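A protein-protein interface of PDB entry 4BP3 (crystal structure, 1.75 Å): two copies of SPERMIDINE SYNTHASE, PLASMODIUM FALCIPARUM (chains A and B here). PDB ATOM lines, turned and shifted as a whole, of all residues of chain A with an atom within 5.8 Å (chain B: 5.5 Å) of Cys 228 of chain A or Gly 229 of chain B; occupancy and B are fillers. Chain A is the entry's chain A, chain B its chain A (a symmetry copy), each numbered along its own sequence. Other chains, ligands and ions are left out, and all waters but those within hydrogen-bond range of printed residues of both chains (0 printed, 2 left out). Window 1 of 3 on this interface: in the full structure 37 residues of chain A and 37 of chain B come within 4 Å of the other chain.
The side-chain hydroxyl (OH) of Tyr 44 of chain B lies within hydrogen-bond range of the side-chain amide nitrogen (NE2) of Gln 16 of chain A, 2.7 Å away. NE1 of Trp 196 of chain A sits at hydrogen-bond distance from OG of Ser 222 of chain B (3.0 Å). The side-chain sulfur (SG) of Cys 228 of chain A lies within hydrogen-bond range of the side-chain hydroxyl (OH) of Tyr 44 of chain B (3.3 Å).
N of Ile 223 of chain A lies within hydrogen-bond range of O of Gly 229 of chain A (3.0 Å). The backbone NH (N) of Trp 196 of chain A lies close to the side-chain hydroxyl (OG) of Ser 194 of chain A. O of Gly 229 of chain B lies within hydrogen-bond range of N of Ile 223 of chain B, 3.0 Å away. The side-chain sulfur of Cys 228 of chain A sits at hydrogen-bond distance from the side-chain amide oxygen of Gln 16 of chain A (3.4 Å).
Among the printed residues, pairs that only touch across the chains: Trp 196 of chain A with Pro 224 of chain B, Pro 224 of chain A with Cys 228 of chain B, Cys 228 of chain A with Pro 224 of chain B, Ile 197 of chain A with Tyr 44 of chain B, Cys 228 of chain A with Gly 229 of chain B and Gly 229 of chain A with Cys 228 of chain B.
Cys 228 of chain A touches just these residues of chain B: Tyr 44, Pro 224 and Gly 229. Of chain A, only Cys 228 (3.96 Å) comes within 4 Å of Gly 229 of chain B. Printed residues of chain B within 4 Å of Pro 224 of chain A: Cys 228 (3.6 Å). Of the printed residues of chain A, Ser 222 of chain B touches Trp 196 (3.0 Å). Of the printed residues of chain A, Tyr 44 of chain B touches Gln 16, Ile 197 and Cys 228. Of the printed residues of chain A, Cys 228 of chain B touches Pro 224 and Gly 229. Thr 225 of chain B touches none of the printed residues of chain A. The nearest residue of chain B that does not touch Cys 228 of chain A is Ile 223 of chain B (4.7 Å). The nearest residue of chain A that does not touch Gly 229 of chain B is Gly 229 of chain A (4.1 Å).
Of the 11 printed residues of chain A, 6 touch a printed residue of chain B. Printed residues of chain A that touch a printed residue of chain B: Gln 16, Trp 196, Ile 197, Pro 224, Cys 228 and Gly 229. Hydrophobic or aromatic side chains of chain A within 4 Å of the printed part of chain B: Trp 196, Ile 197 and Pro 224. Of the 12 printed residues of chain B, 5 touch a printed residue of chain A.
Pro 224 of chain A touches Cys 228 of chain B, and with the chains exchanged Cys 228 of chain A touches Pro 224 of chain B. Cys 228 of chain A touches Gly 229 of chain B, and with the chains exchanged Gly 229 of chain A touches Cys 228 of chain B. Of the 9 pairs that touch across the chains among the printed residues, 4 have their exchanged pair printed and touching as well.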
ATOM      1  N   GLN A  16      -0.725  16.579  20.556  1.00  0.00           N
ATOM      2  CA  GLN A  16      -0.836  17.690  19.648  1.00  0.00           C
ATOM      3  C   GLN A  16      -0.030  18.878  20.085  1.00  0.00           C
ATOM      4  O   GLN A  16       0.244  19.014  21.250  1.00  0.00           O
ATOM      5  CB  GLN A  16      -2.298  18.110  19.489  1.00  0.00           C
ATOM      6  CG  GLN A  16      -2.839  18.961  20.600  1.00  0.00           C
ATOM      7  CD  GLN A  16      -4.282  19.318  20.431  1.00  0.00           C
ATOM      8  OE1 GLN A  16      -4.618  20.516  20.138  1.00  0.00           O
ATOM      9  NE2 GLN A  16      -5.158  18.354  20.671  1.00  0.00           N
ATOM     10  N   SER A 194     -11.463  24.053  25.275  1.00  0.00           N
ATOM     11  CA  SER A 194     -11.791  23.672  23.929  1.00  0.00           C
ATOM     12  C   SER A 194     -12.718  22.471  23.834  1.00  0.00           C
ATOM     13  O   SER A 194     -12.434  21.407  24.352  1.00  0.00           O
ATOM     14  CB  SER A 194     -10.538  23.279  23.235  1.00  0.00           C
ATOM     15  OG  SER A 194     -10.823  23.060  21.880  1.00  0.00           O
ATOM     16  N   TRP A 196     -13.085  20.449  21.534  1.00  0.00           N
ATOM     17  CA  TRP A 196     -12.535  19.277  20.803  1.00  0.00           C
ATOM     18  C   TRP A 196     -11.824  18.268  21.685  1.00  0.00           C
ATOM     19  O   TRP A 196     -11.704  17.070  21.341  1.00  0.00           O
ATOM     20  CB  TRP A 196     -11.666  19.794  19.707  1.00  0.00           C
ATOM     21  CG  TRP A 196     -12.424  20.194  18.650  1.00  0.00           C
ATOM     22  CD1 TRP A 196     -12.694  21.479  18.221  1.00  0.00           C
ATOM     23  CD2 TRP A 196     -13.096  19.319  17.749  1.00  0.00           C
ATOM     24  NE1 TRP A 196     -13.537  21.435  17.141  1.00  0.00           N
ATOM     25  CE2 TRP A 196     -13.773  20.124  16.817  1.00  0.00           C
ATOM     26  CE3 TRP A 196     -13.163  17.938  17.642  1.00  0.00           C
ATOM     27  CZ2 TRP A 196     -14.501  19.605  15.779  1.00  0.00           C
ATOM     28  CZ3 TRP A 196     -13.907  17.413  16.551  1.00  0.00           C
ATOM     29  CH2 TRP A 196     -14.549  18.225  15.680  1.00  0.00           C
ATOM     30  N   ILE A 197     -11.318  18.717  22.836  1.00  0.00           N
ATOM     31  CA  ILE A 197     -10.490  17.865  23.640  1.00  0.00           C
ATOM     32  C   ILE A 197     -10.746  17.938  25.099  1.00  0.00           C
ATOM     33  O   ILE A 197     -10.272  17.088  25.824  1.00  0.00           O
ATOM     34  CB  ILE A 197      -8.992  18.161  23.450  1.00  0.00           C
ATOM     35  CG1 ILE A 197      -8.698  19.703  23.564  1.00  0.00           C
ATOM     36  CG2 ILE A 197      -8.521  17.508  22.157  1.00  0.00           C
ATOM     37  CD1 ILE A 197      -7.240  20.088  23.468  1.00  0.00           C
ATOM     38  N   ILE A 223     -10.249  31.262  17.422  1.00  0.00           N
ATOM     39  CA  ILE A 223      -9.027  31.946  17.647  1.00  0.00           C
ATOM     40  C   ILE A 223      -7.869  30.994  17.502  1.00  0.00           C
ATOM     41  O   ILE A 223      -7.776  29.980  18.219  1.00  0.00           O
ATOM     42  CB  ILE A 223      -9.000  32.647  19.005  1.00  0.00           C
ATOM     43  CG1 ILE A 223      -7.603  33.151  19.365  1.00  0.00           C
ATOM     44  CG2 ILE A 223      -9.520  31.768  20.128  1.00  0.00           C
ATOM     45  CD1 ILE A 223      -7.609  34.290  20.390  1.00  0.00           C
ATOM     46  N   PRO A 224      -6.997  31.343  16.587  1.00  0.00           N
ATOM     47  CA  PRO A 224      -6.087  30.292  16.086  1.00  0.00           C
ATOM     48  C   PRO A 224      -5.006  29.892  17.035  1.00  0.00           C
ATOM     49  O   PRO A 224      -4.553  28.748  16.984  1.00  0.00           O
ATOM     50  CB  PRO A 224      -5.466  30.916  14.887  1.00  0.00           C
ATOM     51  CG  PRO A 224      -5.758  32.373  14.997  1.00  0.00           C
ATOM     52  CD  PRO A 224      -7.017  32.492  15.697  1.00  0.00           C
ATOM     53  N   TYR A 226      -5.112  29.561  20.398  1.00  0.00           N
ATOM     54  CA  TYR A 226      -5.395  28.678  21.454  1.00  0.00           C
ATOM     55  C   TYR A 226      -5.592  27.230  20.895  1.00  0.00           C
ATOM     56  O   TYR A 226      -5.964  27.027  19.729  1.00  0.00           O
ATOM     57  CB  TYR A 226      -6.620  29.093  22.268  1.00  0.00           C
ATOM     58  CG  TYR A 226      -6.473  30.422  22.982  1.00  0.00           C
ATOM     59  CD1 TYR A 226      -5.316  30.724  23.708  1.00  0.00           C
ATOM     60  CD2 TYR A 226      -7.515  31.277  23.056  1.00  0.00           C
ATOM     61  CE1 TYR A 226      -5.201  31.903  24.431  1.00  0.00           C
ATOM     62  CE2 TYR A 226      -7.395  32.488  23.730  1.00  0.00           C
ATOM     63  CZ  TYR A 226      -6.227  32.820  24.415  1.00  0.00           C
ATOM     64  OH  TYR A 226      -6.076  34.056  25.071  1.00  0.00           O
ATOM     65  N   PRO A 227      -5.378  26.228  21.739  1.00  0.00           N
ATOM     66  CA  PRO A 227      -5.316  24.815  21.241  1.00  0.00           C
ATOM     67  C   PRO A 227      -6.629  24.362  20.619  1.00  0.00           C
ATOM     68  O   PRO A 227      -7.703  24.673  21.131  1.00  0.00           O
ATOM     69  CB  PRO A 227      -5.139  24.021  22.507  1.00  0.00           C
ATOM     70  CG  PRO A 227      -4.268  24.941  23.328  1.00  0.00           C
ATOM     71  CD  PRO A 227      -4.803  26.327  23.081  1.00  0.00           C
ATOM     72  N   CYS A 228      -6.513  23.713  19.475  1.00  0.00           N
ATOM     73  CA  CYS A 228      -7.668  23.304  18.682  1.00  0.00           C
ATOM     74  C   CYS A 228      -8.322  24.460  17.949  1.00  0.00           C
ATOM     75  O   CYS A 228      -9.281  24.243  17.207  1.00  0.00           O
ATOM     76  CB  CYS A 228      -8.645  22.481  19.493  1.00  0.00           C
ATOM     77  SG  CYS A 228      -8.037  20.840  19.999  1.00  0.00           S
ATOM     78  N   GLY A 229      -7.739  25.669  18.052  1.00  0.00           N
ATOM     79  CA  GLY A 229      -8.209  26.880  17.384  1.00  0.00           C
ATOM     80  C   GLY A 229      -9.538  27.455  17.836  1.00  0.00           C
ATOM     81  O   GLY A 229     -10.128  28.277  17.148  1.00  0.00           O
ATOM     82  N   CYS A 230      -9.936  27.105  19.028  1.00  0.00           N
ATOM     83  CA  CYS A 230     -11.150  27.648  19.571  1.00  0.00           C
ATOM     84  C   CYS A 230     -11.018  27.651  21.102  1.00  0.00           C
ATOM     85  O   CYS A 230     -10.257  26.905  21.737  1.00  0.00           O
ATOM     86  CB  CYS A 230     -12.385  26.841  19.103  1.00  0.00           C
ATOM     87  SG  CYS A 230     -12.519  25.157  19.747  1.00  0.00           S
ATOM     88  N   TYR B  44      -5.548  11.375  17.811  1.00  0.00           N
ATOM     89  CA  TYR B  44      -6.524  11.744  16.806  1.00  0.00           C
ATOM     90  C   TYR B  44      -6.886  10.611  15.836  1.00  0.00           C
ATOM     91  O   TYR B  44      -7.559  10.855  14.799  1.00  0.00           O
ATOM     92  CB  TYR B  44      -6.069  12.986  16.019  1.00  0.00           C
ATOM     93  CG  TYR B  44      -6.288  14.319  16.770  1.00  0.00           C
ATOM     94  CD1 TYR B  44      -5.626  14.601  17.952  1.00  0.00           C
ATOM     95  CD2 TYR B  44      -7.112  15.310  16.249  1.00  0.00           C
ATOM     96  CE1 TYR B  44      -5.838  15.839  18.645  1.00  0.00           C
ATOM     97  CE2 TYR B  44      -7.333  16.536  16.902  1.00  0.00           C
ATOM     98  CZ  TYR B  44      -6.693  16.792  18.098  1.00  0.00           C
ATOM     99  OH  TYR B  44      -6.949  18.022  18.690  1.00  0.00           O
ATOM    100  N   ILE B 221     -16.143  26.643   9.749  1.00  0.00           N
ATOM    101  CA  ILE B 221     -16.256  25.375  10.548  1.00  0.00           C
ATOM    102  C   ILE B 221     -15.121  25.313  11.538  1.00  0.00           C
ATOM    103  O   ILE B 221     -14.036  25.645  11.199  1.00  0.00           O
ATOM    104  CB  ILE B 221     -16.050  24.157   9.585  1.00  0.00           C
ATOM    105  CG1 ILE B 221     -17.032  24.191   8.438  1.00  0.00           C
ATOM    106  CG2 ILE B 221     -16.277  22.848  10.262  1.00  0.00           C
ATOM    107  CD1 ILE B 221     -16.686  23.184   7.359  1.00  0.00           C
ATOM    108  N   SER B 222     -15.391  24.871  12.758  1.00  0.00           N
ATOM    109  CA  SER B 222     -14.353  24.619  13.700  1.00  0.00           C
ATOM    110  C   SER B 222     -13.913  23.163  13.438  1.00  0.00           C
ATOM    111  O   SER B 222     -14.712  22.173  13.531  1.00  0.00           O
ATOM    112  CB  SER B 222     -14.903  24.749  15.085  1.00  0.00           C
ATOM    113  OG  SER B 222     -14.097  24.143  16.056  1.00  0.00           O
ATOM    114  N   ILE B 223     -12.619  23.057  13.196  1.00  0.00           N
ATOM    115  CA  ILE B 223     -11.992  21.792  13.062  1.00  0.00           C
ATOM    116  C   ILE B 223     -10.517  21.916  13.337  1.00  0.00           C
ATOM    117  O   ILE B 223      -9.798  22.675  12.660  1.00  0.00           O
ATOM    118  CB  ILE B 223     -12.249  21.163  11.693  1.00  0.00           C
ATOM    119  CG1 ILE B 223     -11.364  19.942  11.445  1.00  0.00           C
ATOM    120  CG2 ILE B 223     -12.071  22.150  10.553  1.00  0.00           C
ATOM    121  CD1 ILE B 223     -11.927  18.982  10.392  1.00  0.00           C
ATOM    122  N   PRO B 224     -10.086  21.158  14.316  1.00  0.00           N
ATOM    123  CA  PRO B 224      -8.788  21.514  14.926  1.00  0.00           C
ATOM    124  C   PRO B 224      -7.593  21.199  14.089  1.00  0.00           C
ATOM    125  O   PRO B 224      -6.575  21.881  14.213  1.00  0.00           O
ATOM    126  CB  PRO B 224      -8.746  20.682  16.158  1.00  0.00           C
ATOM    127  CG  PRO B 224      -9.805  19.650  15.981  1.00  0.00           C
ATOM    128  CD  PRO B 224     -10.838  20.252  15.168  1.00  0.00           C
ATOM    129  N   THR B 225      -7.734  20.232  13.170  1.00  0.00           N
ATOM    130  CA  THR B 225      -6.595  19.774  12.386  1.00  0.00           C
ATOM    131  C   THR B 225      -6.450  20.378  11.041  1.00  0.00           C
ATOM    132  O   THR B 225      -5.636  19.897  10.276  1.00  0.00           O
ATOM    133  CB  THR B 225      -6.550  18.238  12.249  1.00  0.00           C
ATOM    134  OG1 THR B 225      -7.720  17.725  11.632  1.00  0.00           O
ATOM    135  CG2 THR B 225      -6.491  17.562  13.577  1.00  0.00           C
ATOM    136  N   TYR B 226      -7.190  21.437  10.741  1.00  0.00           N
ATOM    137  CA  TYR B 226      -6.821  22.293   9.689  1.00  0.00           C
ATOM    138  C   TYR B 226      -6.205  23.609  10.268  1.00  0.00           C
ATOM    139  O   TYR B 226      -6.498  24.021  11.402  1.00  0.00           O
ATOM    140  CB  TYR B 226      -7.985  22.629   8.757  1.00  0.00           C
ATOM    141  CG  TYR B 226      -8.560  21.434   8.022  1.00  0.00           C
ATOM    142  CD1 TYR B 226      -7.723  20.505   7.394  1.00  0.00           C
ATOM    143  CD2 TYR B 226      -9.891  21.325   7.831  1.00  0.00           C
ATOM    144  CE1 TYR B 226      -8.237  19.452   6.652  1.00  0.00           C
ATOM    145  CE2 TYR B 226     -10.425  20.244   7.137  1.00  0.00           C
ATOM    146  CZ  TYR B 226      -9.599  19.285   6.550  1.00  0.00           C
ATOM    147  OH  TYR B 226     -10.123  18.167   5.875  1.00  0.00           O
ATOM    148  N   PRO B 227      -5.384  24.286   9.475  1.00  0.00           N
ATOM    149  CA  PRO B 227      -4.571  25.424  10.017  1.00  0.00           C
ATOM    150  C   PRO B 227      -5.440  26.563  10.531  1.00  0.00           C
ATOM    151  O   PRO B 227      -6.448  26.906   9.917  1.00  0.00           O
ATOM    152  CB  PRO B 227      -3.860  25.939   8.795  1.00  0.00           C
ATOM    153  CG  PRO B 227      -3.601  24.663   8.030  1.00  0.00           C
ATOM    154  CD  PRO B 227      -4.850  23.839   8.189  1.00  0.00           C
ATOM    155  N   CYS B 228      -5.077  27.061  11.699  1.00  0.00           N
ATOM    156  CA  CYS B 228      -5.858  28.078  12.396  1.00  0.00           C
ATOM    157  C   CYS B 228      -7.117  27.524  13.035  1.00  0.00           C
ATOM    158  O   CYS B 228      -7.842  28.270  13.694  1.00  0.00           O
ATOM    159  CB  CYS B 228      -6.112  29.289  11.525  1.00  0.00           C
ATOM    160  SG  CYS B 228      -4.635  30.274  11.121  1.00  0.00           S
ATOM    161  N   GLY B 229      -7.321  26.196  12.951  1.00  0.00           N
ATOM    162  CA  GLY B 229      -8.456  25.489  13.540  1.00  0.00           C
ATOM    163  C   GLY B 229      -9.829  25.764  12.955  1.00  0.00           C
ATOM    164  O   GLY B 229     -10.841  25.445  13.563  1.00  0.00           O
ATOM    165  N   CYS B 230      -9.847  26.244  11.742  1.00  0.00           N
ATOM    166  CA  CYS B 230     -11.099  26.476  11.078  1.00  0.00           C
ATOM    167  C   CYS B 230     -10.856  26.355   9.564  1.00  0.00           C
ATOM    168  O   CYS B 230      -9.752  26.516   9.022  1.00  0.00           O
ATOM    169  CB  CYS B 230     -11.688  27.857  11.455  1.00  0.00           C
ATOM    170  SG  CYS B 230     -10.780  29.297  10.850  1.00  0.00           S
ATOM    171  N   ILE B 231     -11.963  26.086   8.882  1.00  0.00           N
ATOM    172  CA  ILE B 231     -11.949  26.090   7.450  1.00  0.00           C
ATOM    173  C   ILE B 231     -13.264  26.632   6.983  1.00  0.00           C
ATOM    174  O   ILE B 231     -14.285  26.356   7.582  1.00  0.00           O
ATOM    175  CB  ILE B 231     -11.685  24.629   6.933  1.00  0.00           C
ATOM    176  CG1 ILE B 231     -11.240  24.710   5.525  1.00  0.00           C
ATOM    177  CG2 ILE B 231     -12.841  23.682   7.225  1.00  0.00           C
ATOM    178  CD1 ILE B 231      -9.830  25.011   5.461  1.00  0.00           C
